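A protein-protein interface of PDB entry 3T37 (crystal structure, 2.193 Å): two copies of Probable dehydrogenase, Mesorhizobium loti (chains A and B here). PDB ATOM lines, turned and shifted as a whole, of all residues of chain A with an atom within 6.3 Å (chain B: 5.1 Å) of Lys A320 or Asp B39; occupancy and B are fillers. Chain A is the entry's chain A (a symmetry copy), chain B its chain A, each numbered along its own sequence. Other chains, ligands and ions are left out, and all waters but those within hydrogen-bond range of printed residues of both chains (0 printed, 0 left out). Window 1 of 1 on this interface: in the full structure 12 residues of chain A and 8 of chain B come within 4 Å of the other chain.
Lys A320 touches two residues of chain B. Asp B39 touches one residue of chain A. Printed residues of chain A within 4 Å of Pro B40: Arg A319 and Lys A320. Of the printed residues of chain B, Pro A321 touches Glu B38 (3.5 Å). Of the printed residues of chain A, Asp B41 touches Arg A319. The nearest residue of chain B that does not touch Lys A320 is Glu B38 (4.3 Å). The nearest residue of chain A that does not touch Asp B39 is Pro A321 (5.0 Å). The nearest printed residue of chain A that does not touch Pro B40 is Pro A321 (5.3 Å).
No position is printed for both chains.
The side-chain carboxylate (OD1) of Asp B39 sits at hydrogen-bond distance from the backbone NH (N) of Asp B41. O of Asp B39 sits at hydrogen-bond distance from ND2 of Asn B225 (3.0 Å). The guanidinium group (NH2) of Arg B35 lies within salt-bridge range of the side-chain carboxylate (OE1) of Glu B38 (3.3 Å). O of Asp B39 lies within hydrogen-bond range of OG of Ser B42, at 3.1 Å. The guanidinium group (NH2) of Arg A319 lies within hydrogen-bond range of the backbone carbonyl oxygen (O) of Gly A432, at 3.0 Å. NE2 of His B524 sits close to OD2 of Asp B39 (3.4 Å).
Of the 11 printed residues of chain A, 3 touch a printed residue of chain B. Hydrophobic or aromatic side chains of chain A within 4 Å of the printed part of chain B: Pro A321. Of the 11 printed residues of chain B, 4 touch a printed residue of chain A. Among the printed residues, 5 pairs touch across the chains.
O of Arg A319 touches CG of Pro B40, 3.7 Å away. Lys A320 touches Pro B40. CD of Pro A321 touches O of Glu B38, at 3.5 Å.
The side-chain carboxylate of Asp B41 is in salt-bridge range of the guanidinium group of Arg A319 (2.5 Å). The side-chain amino group (NZ) of Lys A320 is in salt-bridge range of the side-chain carboxylate (OD2) of Asp B39 (3.99 Å).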
ATOM      1  N   ALA A 318       5.991   5.560  -1.619  1.00  0.00           N
ATOM      2  CA  ALA A 318       5.342   5.563  -0.311  1.00  0.00           C
ATOM      3  C   ALA A 318       6.290   5.887   0.849  1.00  0.00           C
ATOM      4  O   ALA A 318       7.440   5.442   0.872  1.00  0.00           O
ATOM      5  CB  ALA A 318       4.623   4.245  -0.072  1.00  0.00           C
ATOM      6  N   ARG A 319       5.784   6.665   1.807  1.00  0.00           N
ATOM      7  CA  ARG A 319       6.519   7.035   3.017  1.00  0.00           C
ATOM      8  C   ARG A 319       6.737   5.835   3.937  1.00  0.00           C
ATOM      9  O   ARG A 319       7.591   5.864   4.828  1.00  0.00           O
ATOM     10  CB  ARG A 319       5.743   8.104   3.791  1.00  0.00           C
ATOM     11  CG  ARG A 319       6.116   9.541   3.455  1.00  0.00           C
ATOM     12  CD  ARG A 319       6.016  10.397   4.724  1.00  0.00           C
ATOM     13  NE  ARG A 319       5.015   9.809   5.592  1.00  0.00           N
ATOM     14  CZ  ARG A 319       5.136   9.641   6.901  1.00  0.00           C
ATOM     15  NH1 ARG A 319       6.219  10.051   7.552  1.00  0.00           N
ATOM     16  NH2 ARG A 319       4.143   9.059   7.560  1.00  0.00           N
ATOM     17  N   LYS A 320       5.946   4.793   3.726  1.00  0.00           N
ATOM     18  CA  LYS A 320       6.017   3.590   4.540  1.00  0.00           C
ATOM     19  C   LYS A 320       5.499   2.410   3.711  1.00  0.00           C
ATOM     20  O   LYS A 320       4.834   2.621   2.695  1.00  0.00           O
ATOM     21  CB  LYS A 320       5.199   3.781   5.820  1.00  0.00           C
ATOM     22  CG  LYS A 320       3.718   4.050   5.608  1.00  0.00           C
ATOM     23  CD  LYS A 320       3.104   4.637   6.883  1.00  0.00           C
ATOM     24  CE  LYS A 320       1.582   4.696   6.811  1.00  0.00           C
ATOM     25  NZ  LYS A 320       1.011   5.236   8.086  1.00  0.00           N
ATOM     26  N   PRO A 321       5.826   1.168   4.121  1.00  0.00           N
ATOM     27  CA  PRO A 321       5.373  -0.032   3.407  1.00  0.00           C
ATOM     28  C   PRO A 321       3.877  -0.084   3.072  1.00  0.00           C
ATOM     29  O   PRO A 321       3.019   0.147   3.926  1.00  0.00           O
ATOM     30  CB  PRO A 321       5.742  -1.161   4.374  1.00  0.00           C
ATOM     31  CG  PRO A 321       6.995  -0.665   5.018  1.00  0.00           C
ATOM     32  CD  PRO A 321       6.818   0.834   5.164  1.00  0.00           C
ATOM     33  N   VAL A 322       3.594  -0.390   1.809  1.00  0.00           N
ATOM     34  CA  VAL A 322       2.243  -0.635   1.327  1.00  0.00           C
ATOM     35  C   VAL A 322       2.019  -2.136   1.418  1.00  0.00           C
ATOM     36  O   VAL A 322       2.772  -2.910   0.823  1.00  0.00           O
ATOM     37  CB  VAL A 322       2.104  -0.213  -0.159  1.00  0.00           C
ATOM     38  CG1 VAL A 322       0.698  -0.450  -0.667  1.00  0.00           C
ATOM     39  CG2 VAL A 322       2.508   1.244  -0.353  1.00  0.00           C
ATOM     40  N   GLY A 369       5.692  -2.986  -2.287  1.00  0.00           N
ATOM     41  CA  GLY A 369       5.612  -2.331  -0.994  1.00  0.00           C
ATOM     42  C   GLY A 369       6.128  -0.898  -0.985  1.00  0.00           C
ATOM     43  O   GLY A 369       5.822  -0.142  -0.063  1.00  0.00           O
ATOM     44  N   SER A 370       6.892  -0.513  -2.007  1.00  0.00           N
ATOM     45  CA  SER A 370       7.573   0.783  -1.999  1.00  0.00           C
ATOM     46  C   SER A 370       6.763   1.933  -2.598  1.00  0.00           C
ATOM     47  O   SER A 370       7.173   3.096  -2.500  1.00  0.00           O
ATOM     48  CB  SER A 370       8.893   0.687  -2.765  1.00  0.00           C
ATOM     49  OG  SER A 370       8.664   0.719  -4.170  1.00  0.00           O
ATOM     50  N   ALA A 371       5.634   1.616  -3.227  1.00  0.00           N
ATOM     51  CA  ALA A 371       4.895   2.618  -4.003  1.00  0.00           C
ATOM     52  C   ALA A 371       3.443   2.224  -4.252  1.00  0.00           C
ATOM     53  O   ALA A 371       3.075   1.056  -4.108  1.00  0.00           O
ATOM     54  CB  ALA A 371       5.608   2.877  -5.336  1.00  0.00           C
ATOM     55  N   GLY A 432       0.300  11.161   4.872  1.00  0.00           N
ATOM     56  CA  GLY A 432       0.844  10.081   5.689  1.00  0.00           C
ATOM     57  C   GLY A 432       1.404   8.947   4.848  1.00  0.00           C
ATOM     58  O   GLY A 432       2.324   8.232   5.275  1.00  0.00           O
ATOM     59  N   TRP A 433       0.860   8.789   3.643  1.00  0.00           N
ATOM     60  CA  TRP A 433       1.292   7.730   2.735  1.00  0.00           C
ATOM     61  C   TRP A 433       2.284   8.199   1.676  1.00  0.00           C
ATOM     62  O   TRP A 433       3.179   7.449   1.279  1.00  0.00           O
ATOM     63  CB  TRP A 433       0.067   7.100   2.067  1.00  0.00           C
ATOM     64  CG  TRP A 433      -0.642   6.191   2.993  1.00  0.00           C
ATOM     65  CD1 TRP A 433      -1.745   6.475   3.757  1.00  0.00           C
ATOM     66  CD2 TRP A 433      -0.273   4.843   3.299  1.00  0.00           C
ATOM     67  NE1 TRP A 433      -2.093   5.372   4.505  1.00  0.00           N
ATOM     68  CE2 TRP A 433      -1.199   4.361   4.248  1.00  0.00           C
ATOM     69  CE3 TRP A 433       0.754   3.995   2.863  1.00  0.00           C
ATOM     70  CZ2 TRP A 433      -1.132   3.063   4.765  1.00  0.00           C
ATOM     71  CZ3 TRP A 433       0.818   2.705   3.377  1.00  0.00           C
ATOM     72  CH2 TRP A 433      -0.119   2.255   4.318  1.00  0.00           C
ATOM     73  N   GLU A 435       5.284   9.782  -0.172  1.00  0.00           N
ATOM     74  CA  GLU A 435       6.643  10.279  -0.027  1.00  0.00           C
ATOM     75  C   GLU A 435       6.884  11.335  -1.092  1.00  0.00           C
ATOM     76  O   GLU A 435       7.370  12.426  -0.792  1.00  0.00           O
ATOM     77  CB  GLU A 435       7.655   9.133  -0.149  1.00  0.00           C
ATOM     78  CG  GLU A 435       9.074   9.569  -0.521  1.00  0.00           C
ATOM     79  CD  GLU A 435       9.932   9.929   0.685  1.00  0.00           C
ATOM     80  OE1 GLU A 435       9.382  10.315   1.746  1.00  0.00           O
ATOM     81  OE2 GLU A 435      11.172   9.823   0.563  1.00  0.00           O
ATOM     82  N   ARG B  35       8.693  -5.653  12.316  1.00  0.00           N
ATOM     83  CA  ARG B  35       7.551  -5.360  11.450  1.00  0.00           C
ATOM     84  C   ARG B  35       6.816  -4.095  11.863  1.00  0.00           C
ATOM     85  O   ARG B  35       6.371  -3.330  11.003  1.00  0.00           O
ATOM     86  CB  ARG B  35       6.589  -6.557  11.348  1.00  0.00           C
ATOM     87  CG  ARG B  35       7.126  -7.727  10.475  1.00  0.00           C
ATOM     88  CD  ARG B  35       6.328  -7.912   9.154  1.00  0.00           C
ATOM     89  NE  ARG B  35       5.853  -6.640   8.644  1.00  0.00           N
ATOM     90  CZ  ARG B  35       4.599  -6.372   8.302  1.00  0.00           C
ATOM     91  NH1 ARG B  35       3.662  -7.299   8.375  1.00  0.00           N
ATOM     92  NH2 ARG B  35       4.293  -5.159   7.869  1.00  0.00           N
ATOM     93  N   LEU B  36       6.699  -3.857  13.167  1.00  0.00           N
ATOM     94  CA  LEU B  36       5.979  -2.675  13.638  1.00  0.00           C
ATOM     95  C   LEU B  36       6.796  -1.402  13.392  1.00  0.00           C
ATOM     96  O   LEU B  36       6.240  -0.345  13.112  1.00  0.00           O
ATOM     97  CB  LEU B  36       5.602  -2.805  15.123  1.00  0.00           C
ATOM     98  CG  LEU B  36       4.676  -3.965  15.481  1.00  0.00           C
ATOM     99  CD1 LEU B  36       4.169  -3.870  16.910  1.00  0.00           C
ATOM    100  CD2 LEU B  36       3.519  -4.036  14.506  1.00  0.00           C
ATOM    101  N   SER B  37       8.118  -1.501  13.471  1.00  0.00           N
ATOM    102  CA  SER B  37       8.939  -0.306  13.319  1.00  0.00           C
ATOM    103  C   SER B  37       9.115   0.069  11.848  1.00  0.00           C
ATOM    104  O   SER B  37       9.778   1.062  11.529  1.00  0.00           O
ATOM    105  CB  SER B  37      10.296  -0.477  13.998  1.00  0.00           C
ATOM    106  OG  SER B  37      11.050  -1.510  13.370  1.00  0.00           O
ATOM    107  N   GLU B  38       8.525  -0.720  10.954  1.00  0.00           N
ATOM    108  CA  GLU B  38       8.474  -0.346   9.539  1.00  0.00           C
ATOM    109  C   GLU B  38       7.652   0.925   9.323  1.00  0.00           C
ATOM    110  O   GLU B  38       7.939   1.692   8.410  1.00  0.00           O
ATOM    111  CB  GLU B  38       7.941  -1.494   8.679  1.00  0.00           C
ATOM    112  CG  GLU B  38       8.893  -2.675   8.628  1.00  0.00           C
ATOM    113  CD  GLU B  38       8.324  -3.858   7.872  1.00  0.00           C
ATOM    114  OE1 GLU B  38       7.208  -3.743   7.313  1.00  0.00           O
ATOM    115  OE2 GLU B  38       8.998  -4.911   7.844  1.00  0.00           O
ATOM    116  N   ASP B  39       6.639   1.143  10.164  1.00  0.00           N
ATOM    117  CA  ASP B  39       5.921   2.414  10.178  1.00  0.00           C
ATOM    118  C   ASP B  39       6.787   3.435  10.904  1.00  0.00           C
ATOM    119  O   ASP B  39       6.920   3.377  12.128  1.00  0.00           O
ATOM    120  CB  ASP B  39       4.583   2.287  10.911  1.00  0.00           C
ATOM    121  CG  ASP B  39       3.756   3.574  10.858  1.00  0.00           C
ATOM    122  OD1 ASP B  39       4.255   4.604  10.337  1.00  0.00           O
ATOM    123  OD2 ASP B  39       2.602   3.561  11.345  1.00  0.00           O
ATOM    124  N   PRO B  40       7.351   4.395  10.157  1.00  0.00           N
ATOM    125  CA  PRO B  40       8.286   5.361  10.746  1.00  0.00           C
ATOM    126  C   PRO B  40       7.577   6.317  11.695  1.00  0.00           C
ATOM    127  O   PRO B  40       8.249   6.975  12.500  1.00  0.00           O
ATOM    128  CB  PRO B  40       8.819   6.117   9.524  1.00  0.00           C
ATOM    129  CG  PRO B  40       7.695   6.053   8.540  1.00  0.00           C
ATOM    130  CD  PRO B  40       7.059   4.696   8.745  1.00  0.00           C
ATOM    131  N   ASP B  41       6.247   6.366  11.620  1.00  0.00           N
ATOM    132  CA  ASP B  41       5.445   7.218  12.499  1.00  0.00           C
ATOM    133  C   ASP B  41       5.140   6.593  13.866  1.00  0.00           C
ATOM    134  O   ASP B  41       4.560   7.245  14.739  1.00  0.00           O
ATOM    135  CB  ASP B  41       4.113   7.574  11.836  1.00  0.00           C
ATOM    136  CG  ASP B  41       4.279   8.435  10.603  1.00  0.00           C
ATOM    137  OD1 ASP B  41       5.390   8.982  10.377  1.00  0.00           O
ATOM    138  OD2 ASP B  41       3.278   8.569   9.860  1.00  0.00           O
ATOM    139  N   SER B  42       5.497   5.328  14.051  1.00  0.00           N
ATOM    140  CA  SER B  42       5.220   4.672  15.326  1.00  0.00           C
ATOM    141  C   SER B  42       6.523   4.343  16.034  1.00  0.00           C
ATOM    142  O   SER B  42       7.428   3.738  15.443  1.00  0.00           O
ATOM    143  CB  SER B  42       4.350   3.420  15.133  1.00  0.00           C
ATOM    144  OG  SER B  42       5.028   2.435  14.388  1.00  0.00           O
ATOM    145  N   ASN B 225      13.245   4.912  15.196  1.00  0.00           N
ATOM    146  CA  ASN B 225      11.983   4.721  15.898  1.00  0.00           C
ATOM    147  C   ASN B 225      11.905   3.384  16.644  1.00  0.00           C
ATOM    148  O   ASN B 225      10.855   3.040  17.195  1.00  0.00           O
ATOM    149  CB  ASN B 225      10.802   4.883  14.929  1.00  0.00           C
ATOM    150  CG  ASN B 225      10.807   3.846  13.820  1.00  0.00           C
ATOM    151  OD1 ASN B 225      11.862   3.462  13.322  1.00  0.00           O
ATOM    152  ND2 ASN B 225       9.619   3.385  13.431  1.00  0.00           N
ATOM    153  N   HIS B 521      -0.811  -2.606  11.453  1.00  0.00           N
ATOM    154  CA  HIS B 521      -0.631  -1.646  10.369  1.00  0.00           C
ATOM    155  C   HIS B 521      -1.975  -1.315   9.722  1.00  0.00           C
ATOM    156  O   HIS B 521      -2.167  -0.222   9.198  1.00  0.00           O
ATOM    157  CB  HIS B 521       0.333  -2.194   9.317  1.00  0.00           C
ATOM    158  CG  HIS B 521       1.761  -2.237   9.761  1.00  0.00           C
ATOM    159  ND1 HIS B 521       2.413  -1.141  10.285  1.00  0.00           N
ATOM    160  CD2 HIS B 521       2.671  -3.243   9.747  1.00  0.00           C
ATOM    161  CE1 HIS B 521       3.658  -1.470  10.581  1.00  0.00           C
ATOM    162  NE2 HIS B 521       3.839  -2.742  10.267  1.00  0.00           N
ATOM    163  N   HIS B 524      -4.791   1.765  12.914  1.00  0.00           N
ATOM    164  CA  HIS B 524      -4.304   2.574  14.046  1.00  0.00           C
ATOM    165  C   HIS B 524      -4.324   4.096  13.789  1.00  0.00           C
ATOM    166  O   HIS B 524      -5.388   4.663  13.520  1.00  0.00           O
ATOM    167  CB  HIS B 524      -2.935   2.097  14.578  1.00  0.00           C
ATOM    168  CG  HIS B 524      -1.814   2.232  13.595  1.00  0.00           C
ATOM    169  ND1 HIS B 524      -0.711   3.027  13.833  1.00  0.00           N
ATOM    170  CD2 HIS B 524      -1.634   1.698  12.364  1.00  0.00           C
ATOM    171  CE1 HIS B 524       0.103   2.968  12.797  1.00  0.00           C
ATOM    172  NE2 HIS B 524      -0.432   2.165  11.890  1.00  0.00           N
